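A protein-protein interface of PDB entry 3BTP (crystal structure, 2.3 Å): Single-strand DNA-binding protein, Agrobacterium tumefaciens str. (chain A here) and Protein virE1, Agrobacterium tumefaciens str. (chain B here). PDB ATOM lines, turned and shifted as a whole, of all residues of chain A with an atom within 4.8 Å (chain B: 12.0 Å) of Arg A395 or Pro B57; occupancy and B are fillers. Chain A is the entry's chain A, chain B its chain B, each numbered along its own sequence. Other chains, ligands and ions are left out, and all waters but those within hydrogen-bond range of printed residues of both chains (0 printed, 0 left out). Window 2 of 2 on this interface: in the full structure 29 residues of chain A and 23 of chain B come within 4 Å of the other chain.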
ATOM      1  N   THR A 350     -13.270  18.247  11.689  1.00  0.00           N
ATOM      2  CA  THR A 350     -14.660  18.092  11.388  1.00  0.00           C
ATOM      3  C   THR A 350     -14.904  16.576  11.065  1.00  0.00           C
ATOM      4  O   THR A 350     -13.980  15.889  10.585  1.00  0.00           O
ATOM      5  CB  THR A 350     -14.906  19.105  10.189  1.00  0.00           C
ATOM      6  OG1 THR A 350     -15.628  20.318  10.625  1.00  0.00           O
ATOM      7  CG2 THR A 350     -15.412  18.522   8.991  1.00  0.00           C
ATOM      8  N   VAL A 351     -16.131  16.056  11.314  1.00  0.00           N
ATOM      9  CA  VAL A 351     -16.482  14.704  10.877  1.00  0.00           C
ATOM     10  C   VAL A 351     -17.759  14.767  10.043  1.00  0.00           C
ATOM     11  O   VAL A 351     -18.720  15.471  10.456  1.00  0.00           O
ATOM     12  CB  VAL A 351     -16.613  13.670  12.074  1.00  0.00           C
ATOM     13  CG1 VAL A 351     -17.796  14.002  13.036  1.00  0.00           C
ATOM     14  CG2 VAL A 351     -16.775  12.256  11.539  1.00  0.00           C
ATOM     15  N   ASN A 352     -17.757  14.051   8.896  1.00  0.00           N
ATOM     16  CA  ASN A 352     -18.898  13.925   8.078  1.00  0.00           C
ATOM     17  C   ASN A 352     -19.916  12.886   8.625  1.00  0.00           C
ATOM     18  O   ASN A 352     -19.601  11.703   8.722  1.00  0.00           O
ATOM     19  CB  ASN A 352     -18.496  13.523   6.635  1.00  0.00           C
ATOM     20  CG  ASN A 352     -19.647  13.732   5.624  1.00  0.00           C
ATOM     21  OD1 ASN A 352     -20.677  14.338   5.925  1.00  0.00           O
ATOM     22  ND2 ASN A 352     -19.453  13.267   4.445  1.00  0.00           N
ATOM     23  N   MET A 353     -21.087  13.370   8.992  1.00  0.00           N
ATOM     24  CA  MET A 353     -22.140  12.626   9.662  1.00  0.00           C
ATOM     25  C   MET A 353     -23.271  12.432   8.678  1.00  0.00           C
ATOM     26  O   MET A 353     -24.214  11.718   8.962  1.00  0.00           O
ATOM     27  CB  MET A 353     -22.643  13.368  10.904  1.00  0.00           C
ATOM     28  CG  MET A 353     -21.585  13.501  11.974  1.00  0.00           C
ATOM     29  SD  MET A 353     -21.826  13.926  13.738  1.00  0.00           S
ATOM     30  CE  MET A 353     -23.212  12.863  14.237  1.00  0.00           C
ATOM     31  N   GLY A 354     -23.144  13.085   7.518  1.00  0.00           N
ATOM     32  CA  GLY A 354     -24.036  12.938   6.396  1.00  0.00           C
ATOM     33  C   GLY A 354     -23.437  11.865   5.509  1.00  0.00           C
ATOM     34  O   GLY A 354     -22.803  10.943   5.990  1.00  0.00           O
ATOM     35  N   ARG A 355     -23.684  11.987   4.202  1.00  0.00           N
ATOM     36  CA  ARG A 355     -23.384  10.942   3.204  1.00  0.00           C
ATOM     37  C   ARG A 355     -23.878   9.521   3.623  1.00  0.00           C
ATOM     38  O   ARG A 355     -23.032   8.670   3.898  1.00  0.00           O
ATOM     39  CB  ARG A 355     -21.879  10.988   2.892  1.00  0.00           C
ATOM     40  CG  ARG A 355     -21.434  10.400   1.601  1.00  0.00           C
ATOM     41  CD  ARG A 355     -19.915  10.379   1.531  1.00  0.00           C
ATOM     42  NE  ARG A 355     -19.391  11.744   1.338  1.00  0.00           N
ATOM     43  CZ  ARG A 355     -18.171  12.073   0.886  1.00  0.00           C
ATOM     44  NH1 ARG A 355     -17.290  11.137   0.527  1.00  0.00           N
ATOM     45  NH2 ARG A 355     -17.830  13.359   0.795  1.00  0.00           N
ATOM     46  N   GLN A 356     -25.210   9.261   3.603  1.00  0.00           N
ATOM     47  CA  GLN A 356     -25.865   7.973   4.136  1.00  0.00           C
ATOM     48  C   GLN A 356     -26.292   6.522   3.470  1.00  0.00           C
ATOM     49  O   GLN A 356     -25.435   5.603   3.549  1.00  0.00           O
ATOM     50  CB  GLN A 356     -26.726   8.286   5.386  1.00  0.00           C
ATOM     51  CG  GLN A 356     -26.005   9.096   6.525  1.00  0.00           C
ATOM     52  CD  GLN A 356     -25.038   8.301   7.517  1.00  0.00           C
ATOM     53  OE1 GLN A 356     -24.928   8.663   8.690  1.00  0.00           O
ATOM     54  NE2 GLN A 356     -24.358   7.259   7.026  1.00  0.00           N
ATOM     55  N   TRP A 383     -20.518   8.055  17.714  1.00  0.00           N
ATOM     56  CA  TRP A 383     -19.524   8.843  16.894  1.00  0.00           C
ATOM     57  C   TRP A 383     -18.277   9.210  17.687  1.00  0.00           C
ATOM     58  O   TRP A 383     -17.167   8.803  17.366  1.00  0.00           O
ATOM     59  CB  TRP A 383     -20.159  10.091  16.264  1.00  0.00           C
ATOM     60  CG  TRP A 383     -21.106   9.728  15.222  1.00  0.00           C
ATOM     61  CD1 TRP A 383     -22.363   9.292  15.411  1.00  0.00           C
ATOM     62  CD2 TRP A 383     -20.868   9.687  13.807  1.00  0.00           C
ATOM     63  NE1 TRP A 383     -22.956   8.980  14.219  1.00  0.00           N
ATOM     64  CE2 TRP A 383     -22.078   9.250  13.203  1.00  0.00           C
ATOM     65  CE3 TRP A 383     -19.749   9.998  12.980  1.00  0.00           C
ATOM     66  CZ2 TRP A 383     -22.235   9.117  11.803  1.00  0.00           C
ATOM     67  CZ3 TRP A 383     -19.889   9.856  11.569  1.00  0.00           C
ATOM     68  CH2 TRP A 383     -21.132   9.417  11.010  1.00  0.00           C
ATOM     69  N   LEU A 392     -13.516   5.818  11.652  1.00  0.00           N
ATOM     70  CA  LEU A 392     -14.219   6.846  10.906  1.00  0.00           C
ATOM     71  C   LEU A 392     -13.232   7.945  10.391  1.00  0.00           C
ATOM     72  O   LEU A 392     -13.647   9.041  10.138  1.00  0.00           O
ATOM     73  CB  LEU A 392     -15.339   7.460  11.792  1.00  0.00           C
ATOM     74  CG  LEU A 392     -16.432   6.619  12.540  1.00  0.00           C
ATOM     75  CD1 LEU A 392     -17.399   7.492  13.308  1.00  0.00           C
ATOM     76  CD2 LEU A 392     -17.214   5.759  11.591  1.00  0.00           C
ATOM     77  N   TRP A 393     -11.940   7.618  10.277  1.00  0.00           N
ATOM     78  CA  TRP A 393     -10.906   8.524   9.807  1.00  0.00           C
ATOM     79  C   TRP A 393     -11.130   8.904   8.361  1.00  0.00           C
ATOM     80  O   TRP A 393     -10.573   9.943   7.933  1.00  0.00           O
ATOM     81  CB  TRP A 393      -9.496   7.889   9.935  1.00  0.00           C
ATOM     82  CG  TRP A 393      -9.409   6.480   9.368  1.00  0.00           C
ATOM     83  CD1 TRP A 393      -9.500   5.322  10.093  1.00  0.00           C
ATOM     84  CD2 TRP A 393      -9.306   6.063   7.977  1.00  0.00           C
ATOM     85  NE1 TRP A 393      -9.414   4.216   9.268  1.00  0.00           N
ATOM     86  CE2 TRP A 393      -9.295   4.633   7.970  1.00  0.00           C
ATOM     87  CE3 TRP A 393      -9.138   6.744   6.760  1.00  0.00           C
ATOM     88  CZ2 TRP A 393      -9.134   3.863   6.774  1.00  0.00           C
ATOM     89  CZ3 TRP A 393      -9.018   5.999   5.567  1.00  0.00           C
ATOM     90  CH2 TRP A 393      -9.029   4.561   5.583  1.00  0.00           C
ATOM     91  N   ASP A 394     -11.885   8.108   7.586  1.00  0.00           N
ATOM     92  CA  ASP A 394     -12.172   8.523   6.215  1.00  0.00           C
ATOM     93  C   ASP A 394     -13.314   9.581   6.128  1.00  0.00           C
ATOM     94  O   ASP A 394     -13.635  10.092   5.043  1.00  0.00           O
ATOM     95  CB  ASP A 394     -12.527   7.346   5.331  1.00  0.00           C
ATOM     96  CG  ASP A 394     -13.880   6.790   5.673  1.00  0.00           C
ATOM     97  OD1 ASP A 394     -14.036   6.311   6.847  1.00  0.00           O
ATOM     98  OD2 ASP A 394     -14.773   6.834   4.783  1.00  0.00           O
ATOM     99  N   ARG A 395     -13.895   9.931   7.280  1.00  0.00           N
ATOM    100  CA  ARG A 395     -14.900  10.964   7.302  1.00  0.00           C
ATOM    101  C   ARG A 395     -14.351  12.260   7.999  1.00  0.00           C
ATOM    102  O   ARG A 395     -15.035  13.241   8.129  1.00  0.00           O
ATOM    103  CB  ARG A 395     -16.127  10.367   7.998  1.00  0.00           C
ATOM    104  CG  ARG A 395     -16.933   9.464   7.104  1.00  0.00           C
ATOM    105  CD  ARG A 395     -18.116   8.854   7.838  1.00  0.00           C
ATOM    106  NE  ARG A 395     -19.014   8.208   6.851  1.00  0.00           N
ATOM    107  CZ  ARG A 395     -20.133   8.713   6.325  1.00  0.00           C
ATOM    108  NH1 ARG A 395     -20.601   9.927   6.680  1.00  0.00           N
ATOM    109  NH2 ARG A 395     -20.825   7.974   5.458  1.00  0.00           N
ATOM    110  N   VAL A 396     -13.092  12.247   8.384  1.00  0.00           N
ATOM    111  CA  VAL A 396     -12.485  13.329   9.155  1.00  0.00           C
ATOM    112  C   VAL A 396     -11.652  14.222   8.239  1.00  0.00           C
ATOM    113  O   VAL A 396     -10.963  13.691   7.356  1.00  0.00           O
ATOM    114  CB  VAL A 396     -11.597  12.755  10.312  1.00  0.00           C
ATOM    115  CG1 VAL A 396     -10.733  13.825  10.951  1.00  0.00           C
ATOM    116  CG2 VAL A 396     -12.507  12.058  11.373  1.00  0.00           C
ATOM    117  N   GLN A 397     -11.769  15.547   8.474  1.00  0.00           N
ATOM    118  CA  GLN A 397     -11.070  16.669   7.771  1.00  0.00           C
ATOM    119  C   GLN A 397     -10.406  17.436   8.862  1.00  0.00           C
ATOM    120  O   GLN A 397     -11.001  17.588   9.890  1.00  0.00           O
ATOM    121  CB  GLN A 397     -12.044  17.695   7.162  1.00  0.00           C
ATOM    122  CG  GLN A 397     -12.563  17.274   5.829  1.00  0.00           C
ATOM    123  CD  GLN A 397     -13.432  18.349   5.144  1.00  0.00           C
ATOM    124  OE1 GLN A 397     -14.394  18.922   5.707  1.00  0.00           O
ATOM    125  NE2 GLN A 397     -13.063  18.648   3.950  1.00  0.00           N
ATOM    126  N   PHE B  50     -29.863  16.346  15.936  1.00  0.00           N
ATOM    127  CA  PHE B  50     -29.247  15.693  14.764  1.00  0.00           C
ATOM    128  C   PHE B  50     -28.169  14.707  15.237  1.00  0.00           C
ATOM    129  O   PHE B  50     -28.163  13.562  14.849  1.00  0.00           O
ATOM    130  CB  PHE B  50     -28.587  16.729  13.773  1.00  0.00           C
ATOM    131  CG  PHE B  50     -27.778  16.038  12.736  1.00  0.00           C
ATOM    132  CD1 PHE B  50     -28.435  15.347  11.668  1.00  0.00           C
ATOM    133  CD2 PHE B  50     -26.396  15.929  12.867  1.00  0.00           C
ATOM    134  CE1 PHE B  50     -27.674  14.607  10.721  1.00  0.00           C
ATOM    135  CE2 PHE B  50     -25.660  15.235  11.964  1.00  0.00           C
ATOM    136  CZ  PHE B  50     -26.289  14.531  10.887  1.00  0.00           C
ATOM    137  N   VAL B  51     -27.332  15.197  16.141  1.00  0.00           N
ATOM    138  CA  VAL B  51     -26.135  14.579  16.583  1.00  0.00           C
ATOM    139  C   VAL B  51     -26.438  13.457  17.607  1.00  0.00           C
ATOM    140  O   VAL B  51     -25.765  12.423  17.577  1.00  0.00           O
ATOM    141  CB  VAL B  51     -25.160  15.773  17.003  1.00  0.00           C
ATOM    142  CG1 VAL B  51     -24.629  15.780  18.464  1.00  0.00           C
ATOM    143  CG2 VAL B  51     -24.191  16.220  15.848  1.00  0.00           C
ATOM    144  N   HIS B  53     -29.214  11.551  17.433  1.00  0.00           N
ATOM    145  CA  HIS B  53     -29.951  10.507  16.718  1.00  0.00           C
ATOM    146  C   HIS B  53     -29.279  10.051  15.416  1.00  0.00           C
ATOM    147  O   HIS B  53     -29.897   9.371  14.603  1.00  0.00           O
ATOM    148  CB  HIS B  53     -31.404  10.957  16.441  1.00  0.00           C
ATOM    149  CG  HIS B  53     -32.169  11.266  17.698  1.00  0.00           C
ATOM    150  ND1 HIS B  53     -32.628  12.536  18.003  1.00  0.00           N
ATOM    151  CD2 HIS B  53     -32.427  10.498  18.793  1.00  0.00           C
ATOM    152  CE1 HIS B  53     -33.151  12.535  19.217  1.00  0.00           C
ATOM    153  NE2 HIS B  53     -33.042  11.312  19.721  1.00  0.00           N
ATOM    154  N   CYS B  54     -28.042  10.448  15.197  1.00  0.00           N
ATOM    155  CA  CYS B  54     -27.360  10.111  13.930  1.00  0.00           C
ATOM    156  C   CYS B  54     -26.773   8.664  13.983  1.00  0.00           C
ATOM    157  O   CYS B  54     -25.928   8.372  14.835  1.00  0.00           O
ATOM    158  CB  CYS B  54     -26.253  11.148  13.559  1.00  0.00           C
ATOM    159  SG  CYS B  54     -25.661  10.978  11.818  1.00  0.00           S
ATOM    160  N   PRO B  55     -27.212   7.792  13.058  1.00  0.00           N
ATOM    161  CA  PRO B  55     -26.714   6.413  12.956  1.00  0.00           C
ATOM    162  C   PRO B  55     -25.264   6.404  12.411  1.00  0.00           C
ATOM    163  O   PRO B  55     -24.911   7.164  11.484  1.00  0.00           O
ATOM    164  CB  PRO B  55     -27.662   5.753  11.920  1.00  0.00           C
ATOM    165  CG  PRO B  55     -28.121   6.876  11.064  1.00  0.00           C
ATOM    166  CD  PRO B  55     -28.189   8.113  11.999  1.00  0.00           C
ATOM    167  N   LEU B  56     -24.449   5.549  13.000  1.00  0.00           N
ATOM    168  CA  LEU B  56     -23.116   5.277  12.492  1.00  0.00           C
ATOM    169  C   LEU B  56     -23.154   4.781  11.041  1.00  0.00           C
ATOM    170  O   LEU B  56     -24.138   4.190  10.622  1.00  0.00           O
ATOM    171  CB  LEU B  56     -22.426   4.286  13.408  1.00  0.00           C
ATOM    172  CG  LEU B  56     -21.861   4.892  14.716  1.00  0.00           C
ATOM    173  CD1 LEU B  56     -21.136   3.827  15.606  1.00  0.00           C
ATOM    174  CD2 LEU B  56     -20.951   6.102  14.483  1.00  0.00           C
ATOM    175  N   PRO B  57     -22.107   5.049  10.251  1.00  0.00           N
ATOM    176  CA  PRO B  57     -22.169   4.471   8.894  1.00  0.00           C
ATOM    177  C   PRO B  57     -22.210   2.916   8.914  1.00  0.00           C
ATOM    178  O   PRO B  57     -22.021   2.315   9.976  1.00  0.00           O
ATOM    179  CB  PRO B  57     -20.895   4.982   8.217  1.00  0.00           C
ATOM    180  CG  PRO B  57     -20.216   5.898   9.247  1.00  0.00           C
ATOM    181  CD  PRO B  57     -20.865   5.797  10.533  1.00  0.00           C
ATOM    182  N   GLU B  58     -22.494   2.283   7.774  1.00  0.00           N
ATOM    183  CA  GLU B  58     -22.347   0.819   7.636  1.00  0.00           C
ATOM    184  C   GLU B  58     -20.925   0.410   7.324  1.00  0.00           C
ATOM    185  O   GLU B  58     -20.446  -0.589   7.868  1.00  0.00           O
ATOM    186  CB  GLU B  58     -23.242   0.265   6.539  1.00  0.00           C
ATOM    187  CG  GLU B  58     -24.433   1.157   6.143  1.00  0.00           C
ATOM    188  CD  GLU B  58     -25.366   0.449   5.137  1.00  0.00           C
ATOM    189  OE1 GLU B  58     -24.852  -0.049   4.092  1.00  0.00           O
ATOM    190  OE2 GLU B  58     -26.604   0.384   5.401  1.00  0.00           O
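Among the printed residues, merely in contact across the chains: Met A353 with Phe B50, Met A353 with Val B51, Gln A356 with Cys B54, Trp A383 with Pro B55, Trp A383 with Leu B56, Trp A383 with Pro B57, Leu A392 with Leu B56, Leu A392 with Pro B57 and Arg A395 with Pro B57.
Of the 14 printed residues of chain A, 5 touch a printed residue of chain B.
Hydrophobic or aromatic side chains of chain A that line the printed part of chain B: Met A353, Trp A383 and Leu A392.
Along chain A the printed residues that touch a printed residue of chain B span positions 353 to 395.
Of the 8 printed residues of chain B, 6 touch a printed residue of chain A.
Hydrophobic or aromatic side chains of chain B that line the printed part of chain A: Phe B50, Val B51, Leu B56 and Pro B57.
Among the printed residues, no Asp or Glu carboxylate lies within 4 Å of a Lys or Arg side-chain nitrogen of the other chain.
OE1 of Gln A356 sits close to O of Met A353.
The guanidinium group (NH1) of Arg A395 sits at hydrogen-bond distance from the backbone carbonyl oxygen (O) of Gly A354, 2.5 Å away.
The backbone carbonyl oxygen (O) of Asn A352 is in hydrogen-bond range of the guanidinium group (NH1) of Arg A395, 2.9 Å away.
The backbone carbonyl oxygen (O) of Arg A355 is in hydrogen-bond range of the guanidinium group (NH2) of Arg A395, 2.8 Å away.
No residue of chain B comes within 4 Å of Thr A350.
No residue of chain B comes within 4 Å of Val A351.
No residue of chain B comes within 4 Å of Asn A352.
Gly A354 touches none of the printed residues of chain B.
Arg A355 touches none of the printed residues of chain B.
Of the printed residues of chain B, Trp A383 touches Cys B54, Pro B55, Leu B56 and Pro B57.
No residue of chain B comes within 4 Å of Asp A394.
No residue of chain B comes within 4 Å of Val A396.
Of the printed residues of chain A, Cys B54 touches Met A353, Gln A356 and Trp A383.
Of the printed residues of chain A, Leu B56 touches Trp A383 (3.5 Å) and Leu A392 (3.99 Å).
Of the printed residues of chain A, Pro B57 touches Trp A383 (3.7 Å), Leu A392 (3.8 Å) and Arg A395 (3.5 Å).
The nearest residue of chain B that does not touch Arg A395 is Glu B58 (6.4 Å).
The nearest printed residue of chain A that does not touch Pro B57 is Gln A356 (4.01 Å).
The nearest printed residue of chain A that does not touch Cys B54 is Gly A354 (5.4 Å).
The backbone carbonyl oxygen (O) of Pro B55 lies close to the side-chain amide oxygen (OE1) of Gln A356, at 3.2 Å.
The indole nitrogen (NE1) of Trp A383 sits at hydrogen-bond distance from the backbone carbonyl oxygen (O) of Cys B54, at 3.1 Å.
The backbone carbonyl oxygen of Met A353 sits at hydrogen-bond distance from the side-chain sulfur of Cys B54, 3.3 Å away.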
